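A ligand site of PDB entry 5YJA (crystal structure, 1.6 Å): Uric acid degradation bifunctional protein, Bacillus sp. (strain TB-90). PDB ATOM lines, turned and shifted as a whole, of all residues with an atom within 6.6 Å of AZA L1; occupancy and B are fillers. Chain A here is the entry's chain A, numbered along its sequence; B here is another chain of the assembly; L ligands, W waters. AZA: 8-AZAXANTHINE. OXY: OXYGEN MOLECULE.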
ATOM      1  N   SER A 182      27.774  -4.796  26.142  1.00  0.00           N
ATOM      2  CA  SER A 182      26.622  -3.942  26.420  1.00  0.00           C
ATOM      3  C   SER A 182      26.944  -2.508  26.053  1.00  0.00           C
ATOM      4  O   SER A 182      28.109  -2.091  25.984  1.00  0.00           O
ATOM      5  CB  SER A 182      26.193  -3.990  27.895  1.00  0.00           C
ATOM      6  OG  SER A 182      27.020  -3.198  28.704  1.00  0.00           O
ATOM      7  N   PHE A 183      25.889  -1.766  25.757  1.00  0.00           N
ATOM      8  CA  PHE A 183      26.020  -0.312  25.631  1.00  0.00           C
ATOM      9  C   PHE A 183      24.734   0.269  26.215  1.00  0.00           C
ATOM     10  O   PHE A 183      23.683   0.301  25.548  1.00  0.00           O
ATOM     11  CB  PHE A 183      26.250   0.160  24.211  1.00  0.00           C
ATOM     12  CG  PHE A 183      26.580   1.618  24.145  1.00  0.00           C
ATOM     13  CD1 PHE A 183      27.703   2.107  24.800  1.00  0.00           C
ATOM     14  CD2 PHE A 183      25.752   2.503  23.472  1.00  0.00           C
ATOM     15  CE1 PHE A 183      28.001   3.474  24.786  1.00  0.00           C
ATOM     16  CE2 PHE A 183      26.047   3.858  23.443  1.00  0.00           C
ATOM     17  CZ  PHE A 183      27.165   4.344  24.114  1.00  0.00           C
ATOM     18  N   PHE A 186      23.828   5.709  28.401  1.00  0.00           N
ATOM     19  CA  PHE A 186      24.132   6.939  27.683  1.00  0.00           C
ATOM     20  C   PHE A 186      22.962   7.923  27.773  1.00  0.00           C
ATOM     21  O   PHE A 186      21.846   7.583  28.197  1.00  0.00           O
ATOM     22  CB  PHE A 186      24.474   6.630  26.224  1.00  0.00           C
ATOM     23  CG  PHE A 186      23.484   5.745  25.519  1.00  0.00           C
ATOM     24  CD1 PHE A 186      23.610   4.349  25.549  1.00  0.00           C
ATOM     25  CD2 PHE A 186      22.425   6.286  24.815  1.00  0.00           C
ATOM     26  CE1 PHE A 186      22.695   3.531  24.880  1.00  0.00           C
ATOM     27  CE2 PHE A 186      21.520   5.476  24.151  1.00  0.00           C
ATOM     28  CZ  PHE A 186      21.647   4.100  24.190  1.00  0.00           C
ATOM     29  N   LEU A 194      18.550   5.594  19.833  1.00  0.00           N
ATOM     30  CA  LEU A 194      19.209   4.310  20.017  1.00  0.00           C
ATOM     31  C   LEU A 194      18.690   3.586  21.242  1.00  0.00           C
ATOM     32  O   LEU A 194      18.820   4.109  22.362  1.00  0.00           O
ATOM     33  CB  LEU A 194      20.707   4.547  20.164  1.00  0.00           C
ATOM     34  CG  LEU A 194      21.605   3.333  20.335  1.00  0.00           C
ATOM     35  CD1 LEU A 194      21.661   2.466  19.061  1.00  0.00           C
ATOM     36  CD2 LEU A 194      22.990   3.803  20.708  1.00  0.00           C
ATOM     37  N   ARG A 200      24.984  -6.859  22.550  1.00  0.00           N
ATOM     38  CA  ARG A 200      25.155  -6.597  21.139  1.00  0.00           C
ATOM     39  C   ARG A 200      26.349  -7.350  20.580  1.00  0.00           C
ATOM     40  O   ARG A 200      27.303  -7.661  21.305  1.00  0.00           O
ATOM     41  CB  ARG A 200      25.371  -5.090  20.877  1.00  0.00           C
ATOM     42  CG  ARG A 200      26.615  -4.532  21.544  1.00  0.00           C
ATOM     43  CD  ARG A 200      26.772  -3.042  21.256  1.00  0.00           C
ATOM     44  NE  ARG A 200      27.957  -2.494  21.903  1.00  0.00           N
ATOM     45  CZ  ARG A 200      28.379  -1.257  21.748  1.00  0.00           C
ATOM     46  NH1 ARG A 200      27.716  -0.423  20.967  1.00  0.00           N
ATOM     47  NH2 ARG A 200      29.464  -0.854  22.375  1.00  0.00           N
ATOM     48  N   LEU A 202      29.234  -6.642  19.104  1.00  0.00           N
ATOM     49  CA  LEU A 202      30.114  -5.516  18.830  1.00  0.00           C
ATOM     50  C   LEU A 202      31.153  -5.852  17.768  1.00  0.00           C
ATOM     51  O   LEU A 202      31.909  -6.826  17.882  1.00  0.00           O
ATOM     52  CB  LEU A 202      30.787  -5.088  20.136  1.00  0.00           C
ATOM     53  CG  LEU A 202      31.772  -3.922  20.042  1.00  0.00           C
ATOM     54  CD1 LEU A 202      31.094  -2.664  19.522  1.00  0.00           C
ATOM     55  CD2 LEU A 202      32.428  -3.643  21.418  1.00  0.00           C
ATOM     56  N   LEU A 246      31.616  -2.652  27.801  1.00  0.00           N
ATOM     57  CA  LEU A 246      30.653  -1.636  28.185  1.00  0.00           C
ATOM     58  C   LEU A 246      30.560  -0.509  27.177  1.00  0.00           C
ATOM     59  O   LEU A 246      29.614   0.287  27.241  1.00  0.00           O
ATOM     60  CB  LEU A 246      31.011  -1.067  29.572  1.00  0.00           C
ATOM     61  CG  LEU A 246      31.062  -2.102  30.697  1.00  0.00           C
ATOM     62  CD1 LEU A 246      31.561  -1.442  31.971  1.00  0.00           C
ATOM     63  CD2 LEU A 246      29.679  -2.698  30.925  1.00  0.00           C
ATOM     64  N   SER A 247      31.488  -0.463  26.223  1.00  0.00           N
ATOM     65  CA  SER A 247      31.606   0.540  25.179  1.00  0.00           C
ATOM     66  C   SER A 247      32.906   0.225  24.474  1.00  0.00           C
ATOM     67  O   SER A 247      33.761  -0.459  25.035  1.00  0.00           O
ATOM     68  CB  SER A 247      31.647   1.959  25.743  1.00  0.00           C
ATOM     69  OG  SER A 247      32.804   2.101  26.560  1.00  0.00           O
ATOM     70  N   ILE A 248      33.067   0.736  23.255  1.00  0.00           N
ATOM     71  CA  ILE A 248      34.365   0.659  22.596  1.00  0.00           C
ATOM     72  C   ILE A 248      35.385   1.480  23.357  1.00  0.00           C
ATOM     73  O   ILE A 248      36.543   1.061  23.509  1.00  0.00           O
ATOM     74  CB  ILE A 248      34.253   1.123  21.134  1.00  0.00           C
ATOM     75  CG1 ILE A 248      33.323   0.209  20.337  1.00  0.00           C
ATOM     76  CG2 ILE A 248      35.638   1.184  20.514  1.00  0.00           C
ATOM     77  CD1 ILE A 248      33.078   0.690  18.900  1.00  0.00           C
ATOM     78  N   GLN A 249      34.981   2.679  23.820  1.00  0.00           N
ATOM     79  CA  GLN A 249      35.838   3.523  24.649  1.00  0.00           C
ATOM     80  C   GLN A 249      36.517   2.723  25.760  1.00  0.00           C
ATOM     81  O   GLN A 249      37.733   2.815  25.948  1.00  0.00           O
ATOM     82  CB  GLN A 249      35.028   4.667  25.275  1.00  0.00           C
ATOM     83  CG  GLN A 249      34.578   5.725  24.275  1.00  0.00           C
ATOM     84  CD  GLN A 249      33.206   5.471  23.691  1.00  0.00           C
ATOM     85  OE1 GLN A 249      32.860   4.355  23.285  1.00  0.00           O
ATOM     86  NE2 GLN A 249      32.401   6.532  23.634  1.00  0.00           N
ATOM     87  N   ASN A 275      33.255   1.766  15.021  1.00  0.00           N
ATOM     88  CA  ASN A 275      32.127   0.885  15.306  1.00  0.00           C
ATOM     89  C   ASN A 275      31.376   0.582  14.020  1.00  0.00           C
ATOM     90  O   ASN A 275      30.875   1.494  13.351  1.00  0.00           O
ATOM     91  CB  ASN A 275      31.194   1.566  16.308  1.00  0.00           C
ATOM     92  CG  ASN A 275      30.198   0.621  16.901  1.00  0.00           C
ATOM     93  OD1 ASN A 275      29.891  -0.421  16.325  1.00  0.00           O
ATOM     94  ND2 ASN A 275      29.676   0.981  18.060  1.00  0.00           N
ATOM     95  N   GLY A 301      30.500   4.985  14.146  1.00  0.00           N
ATOM     96  CA  GLY A 301      31.112   5.637  15.275  1.00  0.00           C
ATOM     97  C   GLY A 301      32.612   5.462  15.256  1.00  0.00           C
ATOM     98  O   GLY A 301      33.151   4.524  14.651  1.00  0.00           O
ATOM     99  N   PHE A 302      33.311   6.379  15.929  1.00  0.00           N
ATOM    100  CA  PHE A 302      34.749   6.237  16.064  1.00  0.00           C
ATOM    101  C   PHE A 302      35.217   6.837  17.379  1.00  0.00           C
ATOM    102  O   PHE A 302      34.534   7.656  18.004  1.00  0.00           O
ATOM    103  CB  PHE A 302      35.511   6.850  14.878  1.00  0.00           C
ATOM    104  CG  PHE A 302      35.322   8.331  14.730  1.00  0.00           C
ATOM    105  CD1 PHE A 302      36.090   9.202  15.464  1.00  0.00           C
ATOM    106  CD2 PHE A 302      34.392   8.836  13.849  1.00  0.00           C
ATOM    107  CE1 PHE A 302      35.921  10.582  15.327  1.00  0.00           C
ATOM    108  CE2 PHE A 302      34.236  10.196  13.712  1.00  0.00           C
ATOM    109  CZ  PHE A 302      34.986  11.064  14.452  1.00  0.00           C
ATOM    110  N   GLN A 303      36.393   6.383  17.799  1.00  0.00           N
ATOM    111  CA  GLN A 303      37.044   6.820  19.038  1.00  0.00           C
ATOM    112  C   GLN A 303      38.536   7.030  18.822  1.00  0.00           C
ATOM    113  O   GLN A 303      39.157   6.275  18.069  1.00  0.00           O
ATOM    114  CB  GLN A 303      36.857   5.784  20.147  1.00  0.00           C
ATOM    115  CG  GLN A 303      35.410   5.508  20.535  1.00  0.00           C
ATOM    116  CD  GLN A 303      34.606   4.630  19.556  1.00  0.00           C
ATOM    117  OE1 GLN A 303      35.163   3.929  18.696  1.00  0.00           O
ATOM    118  NE2 GLN A 303      33.295   4.669  19.696  1.00  0.00           N
ATOM    119  N   TYR B  10      35.678  11.210  20.468  1.00  0.00           N
ATOM    120  CA  TYR B  10      34.824  10.207  19.830  1.00  0.00           C
ATOM    121  C   TYR B  10      33.770  10.934  19.004  1.00  0.00           C
ATOM    122  O   TYR B  10      33.561  12.146  19.122  1.00  0.00           O
ATOM    123  CB  TYR B  10      34.205   9.259  20.864  1.00  0.00           C
ATOM    124  CG  TYR B  10      32.999   9.812  21.583  1.00  0.00           C
ATOM    125  CD1 TYR B  10      33.100  10.888  22.429  1.00  0.00           C
ATOM    126  CD2 TYR B  10      31.753   9.228  21.388  1.00  0.00           C
ATOM    127  CE1 TYR B  10      31.999  11.385  23.081  1.00  0.00           C
ATOM    128  CE2 TYR B  10      30.639   9.710  22.028  1.00  0.00           C
ATOM    129  CZ  TYR B  10      30.769  10.791  22.865  1.00  0.00           C
ATOM    130  OH  TYR B  10      29.645  11.310  23.490  1.00  0.00           O
ATOM    131  N   GLY B  11      33.146  10.201  18.094  1.00  0.00           N
ATOM    132  CA  GLY B  11      32.244  10.839  17.167  1.00  0.00           C
ATOM    133  C   GLY B  11      31.680   9.894  16.142  1.00  0.00           C
ATOM    134  O   GLY B  11      31.653   8.676  16.345  1.00  0.00           O
ATOM    135  N   LYS B  12      31.190  10.487  15.053  1.00  0.00           N
ATOM    136  CA  LYS B  12      30.510   9.768  13.976  1.00  0.00           C
ATOM    137  C   LYS B  12      31.006  10.256  12.632  1.00  0.00           C
ATOM    138  O   LYS B  12      31.094  11.466  12.385  1.00  0.00           O
ATOM    139  CB  LYS B  12      28.990   9.970  14.080  1.00  0.00           C
ATOM    140  CG  LYS B  12      28.166   8.927  13.351  1.00  0.00           C
ATOM    141  CD  LYS B  12      28.059   7.680  14.210  1.00  0.00           C
ATOM    142  CE  LYS B  12      26.949   6.796  13.826  1.00  0.00           C
ATOM    143  NZ  LYS B  12      26.790   5.733  14.846  1.00  0.00           N
ATOM    144  N   ASN B  66      28.817   5.505  31.034  1.00  0.00           N
ATOM    145  CA  ASN B  66      28.316   6.204  29.864  1.00  0.00           C
ATOM    146  C   ASN B  66      27.390   7.374  30.209  1.00  0.00           C
ATOM    147  O   ASN B  66      26.822   7.985  29.314  1.00  0.00           O
ATOM    148  CB  ASN B  66      27.581   5.216  28.945  1.00  0.00           C
ATOM    149  CG  ASN B  66      28.532   4.219  28.304  1.00  0.00           C
ATOM    150  OD1 ASN B  66      29.593   4.605  27.830  1.00  0.00           O
ATOM    151  ND2 ASN B  66      28.147   2.941  28.291  1.00  0.00           N
ATOM    152  N   VAL B  69      27.885  10.320  28.105  1.00  0.00           N
ATOM    153  CA  VAL B  69      28.113  10.027  26.695  1.00  0.00           C
ATOM    154  C   VAL B  69      26.879  10.406  25.895  1.00  0.00           C
ATOM    155  O   VAL B  69      25.804   9.859  26.113  1.00  0.00           O
ATOM    156  CB  VAL B  69      28.452   8.542  26.482  1.00  0.00           C
ATOM    157  CG1 VAL B  69      28.485   8.202  25.004  1.00  0.00           C
ATOM    158  CG2 VAL B  69      29.768   8.178  27.150  1.00  0.00           C
ATOM    159  N   VAL B  70      27.036  11.364  24.982  1.00  0.00           N
ATOM    160  CA  VAL B  70      26.109  11.511  23.866  1.00  0.00           C
ATOM    161  C   VAL B  70      26.390  10.381  22.897  1.00  0.00           C
ATOM    162  O   VAL B  70      27.499  10.284  22.367  1.00  0.00           O
ATOM    163  CB  VAL B  70      26.275  12.879  23.183  1.00  0.00           C
ATOM    164  CG1 VAL B  70      25.329  13.033  22.014  1.00  0.00           C
ATOM    165  CG2 VAL B  70      26.129  14.040  24.193  1.00  0.00           C
ATOM    166  N   ALA B  71      25.411   9.489  22.684  1.00  0.00           N
ATOM    167  CA  ALA B  71      25.640   8.407  21.739  1.00  0.00           C
ATOM    168  C   ALA B  71      26.010   8.952  20.362  1.00  0.00           C
ATOM    169  O   ALA B  71      25.507   9.994  19.913  1.00  0.00           O
ATOM    170  CB  ALA B  71      24.419   7.509  21.631  1.00  0.00           C
ATOM    171  N   THR B  72      26.909   8.266  19.680  1.00  0.00           N
ATOM    172  CA  THR B  72      27.263   8.750  18.354  1.00  0.00           C
ATOM    173  C   THR B  72      26.071   8.691  17.402  1.00  0.00           C
ATOM    174  O   THR B  72      25.927   9.566  16.537  1.00  0.00           O
ATOM    175  CB  THR B  72      28.439   7.954  17.782  1.00  0.00           C
ATOM    176  OG1 THR B  72      28.012   6.619  17.512  1.00  0.00           O
ATOM    177  CG2 THR B  72      29.613   7.931  18.738  1.00  0.00           C
ATOM    178  N   ASP B  73      25.192   7.703  17.580  1.00  0.00           N
ATOM    179  CA  ASP B  73      23.927   7.686  16.853  1.00  0.00           C
ATOM    180  C   ASP B  73      23.144   8.978  17.074  1.00  0.00           C
ATOM    181  O   ASP B  73      22.522   9.517  16.144  1.00  0.00           O
ATOM    182  CB  ASP B  73      23.096   6.471  17.264  1.00  0.00           C
ATOM    183  CG  ASP B  73      21.904   6.259  16.368  1.00  0.00           C
ATOM    184  OD1 ASP B  73      22.094   5.803  15.221  1.00  0.00           O
ATOM    185  OD2 ASP B  73      20.785   6.596  16.788  1.00  0.00           O
ATOM    186  N   SER B  74      23.158   9.501  18.295  1.00  0.00           N
ATOM    187  CA  SER B  74      22.455  10.755  18.582  1.00  0.00           C
ATOM    188  C   SER B  74      23.110  11.950  17.912  1.00  0.00           C
ATOM    189  O   SER B  74      22.401  12.886  17.498  1.00  0.00           O
ATOM    190  CB  SER B  74      22.385  10.985  20.088  1.00  0.00           C
ATOM    191  OG  SER B  74      21.798   9.852  20.735  1.00  0.00           O
ATOM    192  N   MET B  75      24.445  11.953  17.799  1.00  0.00           N
ATOM    193  CA  MET B  75      25.134  12.967  16.982  1.00  0.00           C
ATOM    194  C   MET B  75      24.649  12.955  15.543  1.00  0.00           C
ATOM    195  O   MET B  75      24.414  14.007  14.943  1.00  0.00           O
ATOM    196  CB  MET B  75      26.641  12.753  17.031  1.00  0.00           C
ATOM    197  CG  MET B  75      27.216  12.847  18.427  1.00  0.00           C
ATOM    198  SD  MET B  75      28.993  12.496  18.389  1.00  0.00           S
ATOM    199  CE  MET B  75      29.324  12.345  20.154  1.00  0.00           C
HETATM  200  N1  AZA L   1      30.363   3.973  22.085  1.00  0.00           N
HETATM  201  C2  AZA L   1      29.978   2.681  21.800  1.00  0.00           C
HETATM  202  O2  AZA L   1      30.651   1.741  22.135  1.00  0.00           O
HETATM  203  N3  AZA L   1      28.829   2.466  21.166  1.00  0.00           N
HETATM  204  C4  AZA L   1      28.036   3.498  20.771  1.00  0.00           C
HETATM  205  C5  AZA L   1      28.417   4.766  21.063  1.00  0.00           C
HETATM  206  C6  AZA L   1      29.603   5.002  21.724  1.00  0.00           C
HETATM  207  O6  AZA L   1      29.980   6.108  21.989  1.00  0.00           O
HETATM  208  N7  AZA L   1      27.458   5.592  20.578  1.00  0.00           N
HETATM  209  N8  AZA L   1      26.511   4.833  19.972  1.00  0.00           N
HETATM  210  N9  AZA L   1      26.862   3.529  20.117  1.00  0.00           N
HETATM  211  O1  OXY L   2      29.779   4.338  18.130  1.00  0.00           O
HETATM  212  O2  OXY L   2      30.783   3.954  18.580  1.00  0.00           O
HETATM  213  O   HOH W   1      25.554   1.464  19.064  1.00  0.00           O
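The backbone NH of Ile 248 lies within hydrogen-bond range of an oxygen (O2) of AZA L1 (2.8 Å). N of Thr 72 of chain B lies within hydrogen-bond range of N7 of AZA L1 (2.9 Å). ND2 of Asn 275 sits at hydrogen-bond distance from O2 of OXY L2 (3.2 Å). A nitrogen (N1) of AZA L1 is in hydrogen-bond range of the side-chain amide oxygen (OE1) of Gln 249, at 2.8 Å. An oxygen (O2) of AZA L1 lies within hydrogen-bond range of the guanidinium group of Arg 200 (2.9 Å). NE2 of Gln 303 sits at hydrogen-bond distance from O2 of OXY L2 (2.8 Å). The side-chain hydroxyl (OG1) of Thr 72 of chain B sits at hydrogen-bond distance from an oxygen (O1) of OXY L2, at 3.0 Å. The side-chain hydroxyl (OG1) of Thr 72 of chain B is in hydrogen-bond range of a nitrogen (N7) of AZA L1 (3.3 Å).
N of Asn 275 is in hydrogen-bond range of O of Gly 301, 2.8 Å away. OH of Tyr 10 of chain B is in hydrogen-bond range of O of Val 70 of chain B. NZ of Lys 12 of chain B lies within hydrogen-bond range of OG1 of Thr 72 of chain B.
Phe 183 touches AZA L1 (CZ to C5, 3.3 Å). CD2 of Leu 194 touches N8 of AZA L1, at 3.7 Å. Ser 247 touches AZA L1 (CA to O2, 3.4 Å). Asn 275 touches AZA L1 (ND2 to N3, 3.5 Å). Gln 303 touches AZA L1. Tyr 10 of chain B touches AZA L1. Val 69 of chain B touches AZA L1. Ala 71 of chain B touches AZA L1 (CA to N7, 3.5 Å). Asp 73 of chain B touches AZA L1 (N to N8, 3.96 Å). Hydrophobic or aromatic side chains within 4 Å of AZA L1: Phe 183, Leu 194, Ile 248, Tyr 10 of chain B, Val 69 of chain B and Ala 71 of chain B. Of the 25 residues printed, 13 come within 4 Å of AZA L1.
Water W1 bridges N9 of AZA L1 (2.7 Å) and NH1 of Arg 200 (3.4 Å).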
